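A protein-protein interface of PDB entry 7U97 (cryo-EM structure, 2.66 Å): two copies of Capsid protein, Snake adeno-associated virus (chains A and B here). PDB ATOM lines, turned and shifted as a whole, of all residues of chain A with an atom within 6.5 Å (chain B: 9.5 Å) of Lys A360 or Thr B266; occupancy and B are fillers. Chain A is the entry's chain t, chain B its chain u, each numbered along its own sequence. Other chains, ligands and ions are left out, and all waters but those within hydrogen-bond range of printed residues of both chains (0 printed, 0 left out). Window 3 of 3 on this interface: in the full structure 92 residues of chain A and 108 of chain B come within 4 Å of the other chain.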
ATOM      1  N   ALA A 228      14.827  13.223   8.792  1.00  0.00           N
ATOM      2  CA  ALA A 228      14.323  13.722  10.064  1.00  0.00           C
ATOM      3  C   ALA A 228      12.817  13.908  10.044  1.00  0.00           C
ATOM      4  O   ALA A 228      12.197  13.961  11.108  1.00  0.00           O
ATOM      5  CB  ALA A 228      15.005  15.039  10.421  1.00  0.00           C
ATOM      6  N   SER A 229      12.221  14.024   8.865  1.00  0.00           N
ATOM      7  CA  SER A 229      10.778  14.114   8.732  1.00  0.00           C
ATOM      8  C   SER A 229      10.116  12.764   8.530  1.00  0.00           C
ATOM      9  O   SER A 229       8.888  12.683   8.610  1.00  0.00           O
ATOM     10  CB  SER A 229      10.413  15.031   7.565  1.00  0.00           C
ATOM     11  OG  SER A 229      10.857  16.354   7.803  1.00  0.00           O
ATOM     12  N   GLY A 230      10.889  11.709   8.298  1.00  0.00           N
ATOM     13  CA  GLY A 230      10.345  10.397   8.029  1.00  0.00           C
ATOM     14  C   GLY A 230      10.404   9.944   6.590  1.00  0.00           C
ATOM     15  O   GLY A 230       9.787   8.929   6.260  1.00  0.00           O
ATOM     16  N   GLN A 358       8.267  -1.083  13.163  1.00  0.00           N
ATOM     17  CA  GLN A 358       8.378   0.351  13.376  1.00  0.00           C
ATOM     18  C   GLN A 358       7.067   1.066  13.071  1.00  0.00           C
ATOM     19  O   GLN A 358       6.179   0.550  12.390  1.00  0.00           O
ATOM     20  CB  GLN A 358       9.443   0.979  12.491  1.00  0.00           C
ATOM     21  CG  GLN A 358       8.989   1.015  11.065  1.00  0.00           C
ATOM     22  CD  GLN A 358       9.800   1.926  10.211  1.00  0.00           C
ATOM     23  OE1 GLN A 358      10.903   2.314  10.567  1.00  0.00           O
ATOM     24  NE2 GLN A 358       9.247   2.292   9.069  1.00  0.00           N
ATOM     25  N   THR A 359       6.970   2.283  13.582  1.00  0.00           N
ATOM     26  CA  THR A 359       5.929   3.254  13.273  1.00  0.00           C
ATOM     27  C   THR A 359       6.444   4.586  13.805  1.00  0.00           C
ATOM     28  O   THR A 359       7.609   4.685  14.204  1.00  0.00           O
ATOM     29  CB  THR A 359       4.575   2.839  13.851  1.00  0.00           C
ATOM     30  OG1 THR A 359       3.558   3.736  13.386  1.00  0.00           O
ATOM     31  CG2 THR A 359       4.601   2.846  15.368  1.00  0.00           C
ATOM     32  N   LYS A 360       5.604   5.624  13.795  1.00  0.00           N
ATOM     33  CA  LYS A 360       6.058   6.938  14.244  1.00  0.00           C
ATOM     34  C   LYS A 360       6.695   6.886  15.626  1.00  0.00           C
ATOM     35  O   LYS A 360       7.786   7.424  15.840  1.00  0.00           O
ATOM     36  CB  LYS A 360       4.907   7.939  14.251  1.00  0.00           C
ATOM     37  CG  LYS A 360       4.379   8.263  12.897  1.00  0.00           C
ATOM     38  CD  LYS A 360       5.512   8.713  12.012  1.00  0.00           C
ATOM     39  CE  LYS A 360       6.050  10.070  12.385  1.00  0.00           C
ATOM     40  NZ  LYS A 360       7.080  10.481  11.397  1.00  0.00           N
ATOM     41  N   GLY A 361       6.027   6.256  16.578  1.00  0.00           N
ATOM     42  CA  GLY A 361       6.545   6.245  17.929  1.00  0.00           C
ATOM     43  C   GLY A 361       7.672   5.263  18.150  1.00  0.00           C
ATOM     44  O   GLY A 361       8.612   5.550  18.893  1.00  0.00           O
ATOM     45  N   THR A 362       7.598   4.105  17.506  1.00  0.00           N
ATOM     46  CA  THR A 362       8.488   2.991  17.797  1.00  0.00           C
ATOM     47  C   THR A 362       9.679   3.022  16.853  1.00  0.00           C
ATOM     48  O   THR A 362       9.507   3.004  15.632  1.00  0.00           O
ATOM     49  CB  THR A 362       7.756   1.661  17.662  1.00  0.00           C
ATOM     50  OG1 THR A 362       7.320   1.502  16.312  1.00  0.00           O
ATOM     51  CG2 THR A 362       6.548   1.635  18.568  1.00  0.00           C
ATOM     52  N   ASN A 363      10.873   3.058  17.414  1.00  0.00           N
ATOM     53  CA  ASN A 363      12.061   2.941  16.596  1.00  0.00           C
ATOM     54  C   ASN A 363      12.321   1.475  16.275  1.00  0.00           C
ATOM     55  O   ASN A 363      12.017   0.597  17.082  1.00  0.00           O
ATOM     56  CB  ASN A 363      13.265   3.524  17.317  1.00  0.00           C
ATOM     57  CG  ASN A 363      13.094   4.982  17.640  1.00  0.00           C
ATOM     58  OD1 ASN A 363      13.366   5.415  18.755  1.00  0.00           O
ATOM     59  ND2 ASN A 363      12.630   5.750  16.669  1.00  0.00           N
ATOM     60  N   ASN B 259      10.310  -3.182   8.214  1.00  0.00           N
ATOM     61  CA  ASN B 259       9.497  -2.550   7.188  1.00  0.00           C
ATOM     62  C   ASN B 259       9.835  -1.076   7.045  1.00  0.00           C
ATOM     63  O   ASN B 259      10.151  -0.389   8.017  1.00  0.00           O
ATOM     64  CB  ASN B 259       8.005  -2.676   7.486  1.00  0.00           C
ATOM     65  CG  ASN B 259       7.594  -1.933   8.731  1.00  0.00           C
ATOM     66  OD1 ASN B 259       8.413  -1.650   9.590  1.00  0.00           O
ATOM     67  ND2 ASN B 259       6.326  -1.596   8.824  1.00  0.00           N
ATOM     68  N   ASN B 261       8.274   2.423   4.687  1.00  0.00           N
ATOM     69  CA  ASN B 261       7.196   2.906   3.838  1.00  0.00           C
ATOM     70  C   ASN B 261       7.762   3.945   2.885  1.00  0.00           C
ATOM     71  O   ASN B 261       8.248   4.991   3.316  1.00  0.00           O
ATOM     72  CB  ASN B 261       6.056   3.485   4.669  1.00  0.00           C
ATOM     73  CG  ASN B 261       4.834   3.783   3.840  1.00  0.00           C
ATOM     74  OD1 ASN B 261       4.925   4.032   2.645  1.00  0.00           O
ATOM     75  ND2 ASN B 261       3.676   3.706   4.460  1.00  0.00           N
ATOM     76  N   SER B 262       7.702   3.649   1.591  1.00  0.00           N
ATOM     77  CA  SER B 262       8.276   4.553   0.608  1.00  0.00           C
ATOM     78  C   SER B 262       7.356   5.729   0.304  1.00  0.00           C
ATOM     79  O   SER B 262       7.820   6.867   0.202  1.00  0.00           O
ATOM     80  CB  SER B 262       8.605   3.781  -0.668  1.00  0.00           C
ATOM     81  OG  SER B 262       7.438   3.213  -1.226  1.00  0.00           O
ATOM     82  N   SER B 263       6.059   5.481   0.145  1.00  0.00           N
ATOM     83  CA  SER B 263       5.150   6.555  -0.241  1.00  0.00           C
ATOM     84  C   SER B 263       4.785   7.457   0.932  1.00  0.00           C
ATOM     85  O   SER B 263       4.922   8.679   0.845  1.00  0.00           O
ATOM     86  CB  SER B 263       3.888   5.969  -0.872  1.00  0.00           C
ATOM     87  OG  SER B 263       4.187   5.305  -2.086  1.00  0.00           O
ATOM     88  N   ASP B 264       4.330   6.877   2.039  1.00  0.00           N
ATOM     89  CA  ASP B 264       3.736   7.651   3.123  1.00  0.00           C
ATOM     90  C   ASP B 264       4.804   8.060   4.126  1.00  0.00           C
ATOM     91  O   ASP B 264       5.496   7.213   4.695  1.00  0.00           O
ATOM     92  CB  ASP B 264       2.629   6.867   3.821  1.00  0.00           C
ATOM     93  CG  ASP B 264       1.390   6.727   2.966  1.00  0.00           C
ATOM     94  OD1 ASP B 264       1.261   7.487   1.982  1.00  0.00           O
ATOM     95  OD2 ASP B 264       0.546   5.857   3.270  1.00  0.00           O
ATOM     96  N   ASN B 265       4.914   9.365   4.351  1.00  0.00           N
ATOM     97  CA  ASN B 265       5.905   9.889   5.277  1.00  0.00           C
ATOM     98  C   ASN B 265       5.538   9.558   6.717  1.00  0.00           C
ATOM     99  O   ASN B 265       6.413   9.266   7.538  1.00  0.00           O
ATOM    100  CB  ASN B 265       6.011  11.399   5.076  1.00  0.00           C
ATOM    101  CG  ASN B 265       7.177  12.002   5.790  1.00  0.00           C
ATOM    102  OD1 ASN B 265       7.747  11.399   6.686  1.00  0.00           O
ATOM    103  ND2 ASN B 265       7.541  13.211   5.403  1.00  0.00           N
ATOM    104  N   THR B 266       4.251   9.570   7.034  1.00  0.00           N
ATOM    105  CA  THR B 266       3.781   9.503   8.409  1.00  0.00           C
ATOM    106  C   THR B 266       3.769   8.094   8.969  1.00  0.00           C
ATOM    107  O   THR B 266       3.326   7.900  10.102  1.00  0.00           O
ATOM    108  CB  THR B 266       2.379  10.093   8.500  1.00  0.00           C
ATOM    109  OG1 THR B 266       1.500   9.348   7.653  1.00  0.00           O
ATOM    110  CG2 THR B 266       2.390  11.531   8.041  1.00  0.00           C
ATOM    111  N   LYS B 267       4.188   7.104   8.196  1.00  0.00           N
ATOM    112  CA  LYS B 267       4.243   5.731   8.663  1.00  0.00           C
ATOM    113  C   LYS B 267       5.629   5.314   9.132  1.00  0.00           C
ATOM    114  O   LYS B 267       5.786   4.190   9.613  1.00  0.00           O
ATOM    115  CB  LYS B 267       3.774   4.790   7.556  1.00  0.00           C
ATOM    116  CG  LYS B 267       2.386   5.088   7.036  1.00  0.00           C
ATOM    117  CD  LYS B 267       1.348   4.936   8.111  1.00  0.00           C
ATOM    118  CE  LYS B 267      -0.038   5.165   7.547  1.00  0.00           C
ATOM    119  NZ  LYS B 267      -1.088   5.059   8.598  1.00  0.00           N
ATOM    120  N   ASN B 268       6.631   6.178   9.009  1.00  0.00           N
ATOM    121  CA  ASN B 268       8.011   5.830   9.304  1.00  0.00           C
ATOM    122  C   ASN B 268       8.495   6.585  10.528  1.00  0.00           C
ATOM    123  O   ASN B 268       8.184   7.764  10.703  1.00  0.00           O
ATOM    124  CB  ASN B 268       8.938   6.160   8.135  1.00  0.00           C
ATOM    125  CG  ASN B 268       8.629   5.368   6.903  1.00  0.00           C
ATOM    126  OD1 ASN B 268       8.542   5.915   5.815  1.00  0.00           O
ATOM    127  ND2 ASN B 268       8.466   4.070   7.061  1.00  0.00           N
ATOM    128  N   ALA B 269       9.282   5.912  11.355  1.00  0.00           N
ATOM    129  CA  ALA B 269       9.929   6.582  12.467  1.00  0.00           C
ATOM    130  C   ALA B 269      10.923   7.608  11.948  1.00  0.00           C
ATOM    131  O   ALA B 269      11.408   7.521  10.820  1.00  0.00           O
ATOM    132  CB  ALA B 269      10.634   5.570  13.365  1.00  0.00           C
ATOM    133  N   ASN B 270      11.222   8.594  12.782  1.00  0.00           N
ATOM    134  CA  ASN B 270      12.098   9.676  12.372  1.00  0.00           C
ATOM    135  C   ASN B 270      13.554   9.292  12.579  1.00  0.00           C
ATOM    136  O   ASN B 270      13.934   8.820  13.654  1.00  0.00           O
ATOM    137  CB  ASN B 270      11.777  10.944  13.155  1.00  0.00           C
ATOM    138  CG  ASN B 270      10.433  11.515  12.802  1.00  0.00           C
ATOM    139  OD1 ASN B 270       9.899  11.258  11.730  1.00  0.00           O
ATOM    140  ND2 ASN B 270       9.870  12.295  13.707  1.00  0.00           N
ATOM    141  N   SER B 271      14.362   9.492  11.538  1.00  0.00           N
ATOM    142  CA  SER B 271      15.819   9.395  11.616  1.00  0.00           C
ATOM    143  C   SER B 271      16.287   7.998  12.009  1.00  0.00           C
ATOM    144  O   SER B 271      17.124   7.833  12.896  1.00  0.00           O
ATOM    145  CB  SER B 271      16.380  10.437  12.584  1.00  0.00           C
ATOM    146  OG  SER B 271      16.151  11.751  12.114  1.00  0.00           O
ATOM    147  N   ILE B 272      15.759   6.985  11.343  1.00  0.00           N
ATOM    148  CA  ILE B 272      16.285   5.645  11.564  1.00  0.00           C
ATOM    149  C   ILE B 272      17.571   5.498  10.770  1.00  0.00           C
ATOM    150  O   ILE B 272      17.759   6.128   9.726  1.00  0.00           O
ATOM    151  CB  ILE B 272      15.270   4.549  11.190  1.00  0.00           C
ATOM    152  CG1 ILE B 272      15.084   4.460   9.688  1.00  0.00           C
ATOM    153  CG2 ILE B 272      13.933   4.838  11.816  1.00  0.00           C
ATOM    154  CD1 ILE B 272      14.237   3.291   9.278  1.00  0.00           C
ATOM    155  N   ALA B 304      -1.642  -0.852   3.817  1.00  0.00           N
ATOM    156  CA  ALA B 304      -1.369   0.565   3.643  1.00  0.00           C
ATOM    157  C   ALA B 304      -0.638   0.791   2.328  1.00  0.00           C
ATOM    158  O   ALA B 304       0.199  -0.015   1.920  1.00  0.00           O
ATOM    159  CB  ALA B 304      -0.538   1.092   4.808  1.00  0.00           C
ATOM    160  N   ALA B 305      -0.967   1.888   1.659  1.00  0.00           N
ATOM    161  CA  ALA B 305      -0.307   2.211   0.405  1.00  0.00           C
ATOM    162  C   ALA B 305       1.121   2.655   0.673  1.00  0.00           C
ATOM    163  O   ALA B 305       1.372   3.466   1.569  1.00  0.00           O
ATOM    164  CB  ALA B 305      -1.074   3.301  -0.333  1.00  0.00           C
ATOM    165  N   GLN B 307       3.602   0.454   1.468  1.00  0.00           N
ATOM    166  CA  GLN B 307       4.275  -0.470   2.367  1.00  0.00           C
ATOM    167  C   GLN B 307       5.356  -1.245   1.627  1.00  0.00           C
ATOM    168  O   GLN B 307       5.148  -1.709   0.504  1.00  0.00           O
ATOM    169  CB  GLN B 307       3.254  -1.428   2.971  1.00  0.00           C
ATOM    170  CG  GLN B 307       3.786  -2.320   4.061  1.00  0.00           C
ATOM    171  CD  GLN B 307       4.245  -1.533   5.267  1.00  0.00           C
ATOM    172  OE1 GLN B 307       3.470  -0.795   5.870  1.00  0.00           O
ATOM    173  NE2 GLN B 307       5.510  -1.683   5.625  1.00  0.00           N
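No position is printed for both chains. Of the 18 pairs that touch across the chains among the printed residues, none has its exchanged pair printed and touching as well.
Hydrophobic or aromatic side chains of chain A that line the printed part of chain B: Ala A228. Hydrophobic or aromatic side chains of chain B within 4 Å of the printed part of chain A: Ala B269 and Ile B272. Among the printed residues, no Asp or Glu carboxylate lies within 4 Å of a Lys or Arg side-chain nitrogen of the other chain.
Among the printed residues, merely in contact across the chains: Lys A360 with Thr B266, Thr A359 with Ala B269, Ala A228 with Ser B271, Ala A228 with Asn B270, Ser A229 with Asn B270, Gly A230 with Asn B270, Thr A362 with Ala B269, Gln A358 with Ile B272, Thr A359 with Lys B267, Asn A363 with Ala B269 and Gln A358 with Lys B267.
N of Thr A359 sits at hydrogen-bond distance from OG1 of Thr A362 (2.9 Å). ND2 of Asn B259 lies close to NE2 of Gln B307 (3.3 Å). The backbone carbonyl oxygen of Asn B261 sits close to the side-chain amide oxygen of Asn B268, at 2.7 Å. The side-chain amide oxygen (OD1) of Asn B268 lies close to the backbone carbonyl oxygen (O) of Asp B264, at 3.5 Å.
The side-chain amide oxygen (OD1) of Asn B265 lies close to the backbone carbonyl oxygen (O) of Ser A229 (2.6 Å). The backbone carbonyl oxygen (O) of Gly A230 lies close to the side-chain amide oxygen (OD1) of Asn B265 (3.2 Å). The backbone carbonyl oxygen of Gly A230 sits close to the side-chain amide oxygen of Asn B268 (3.3 Å). The backbone carbonyl oxygen (O) of Asn B259 sits at hydrogen-bond distance from the side-chain amide nitrogen (NE2) of Gln A358 (3.0 Å). The side-chain amide nitrogen (ND2) of Asn B268 sits close to the side-chain amide nitrogen (NE2) of Gln A358 (2.8 Å). The backbone carbonyl oxygen of Asn B268 lies within hydrogen-bond range of the side-chain amino group of Lys A360. The side-chain amide oxygen (OD1) of Asn B270 is in hydrogen-bond range of the side-chain amino group (NZ) of Lys A360.
Lys A360 touches just these residues of chain B: Thr B266 (3.0 Å), Asn B268 (3.0 Å) and Asn B270 (2.9 Å). Thr A359 touches just these residues of chain B: Lys B267 (3.8 Å) and Ala B269 (3.3 Å). No residue of chain B comes within 4 Å of Gly A361. Printed residues of chain A within 4 Å of Ser B271: Ala A228. Of the printed residues of chain B, Thr A362 touches Ala B269 (3.6 Å). Of the printed residues of chain B, Ala A228 touches Asn B270 and Ser B271. Printed residues of chain A within 4 Å of Asn B265: Ser A229 and Gly A230. Ser B262 touches none of the printed residues of chain A. The nearest printed residue of chain B that does not touch Lys A360 is Ala B269 (4.1 Å). The nearest residue of chain A that does not touch Thr B266 is Thr A359 (5.3 Å).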
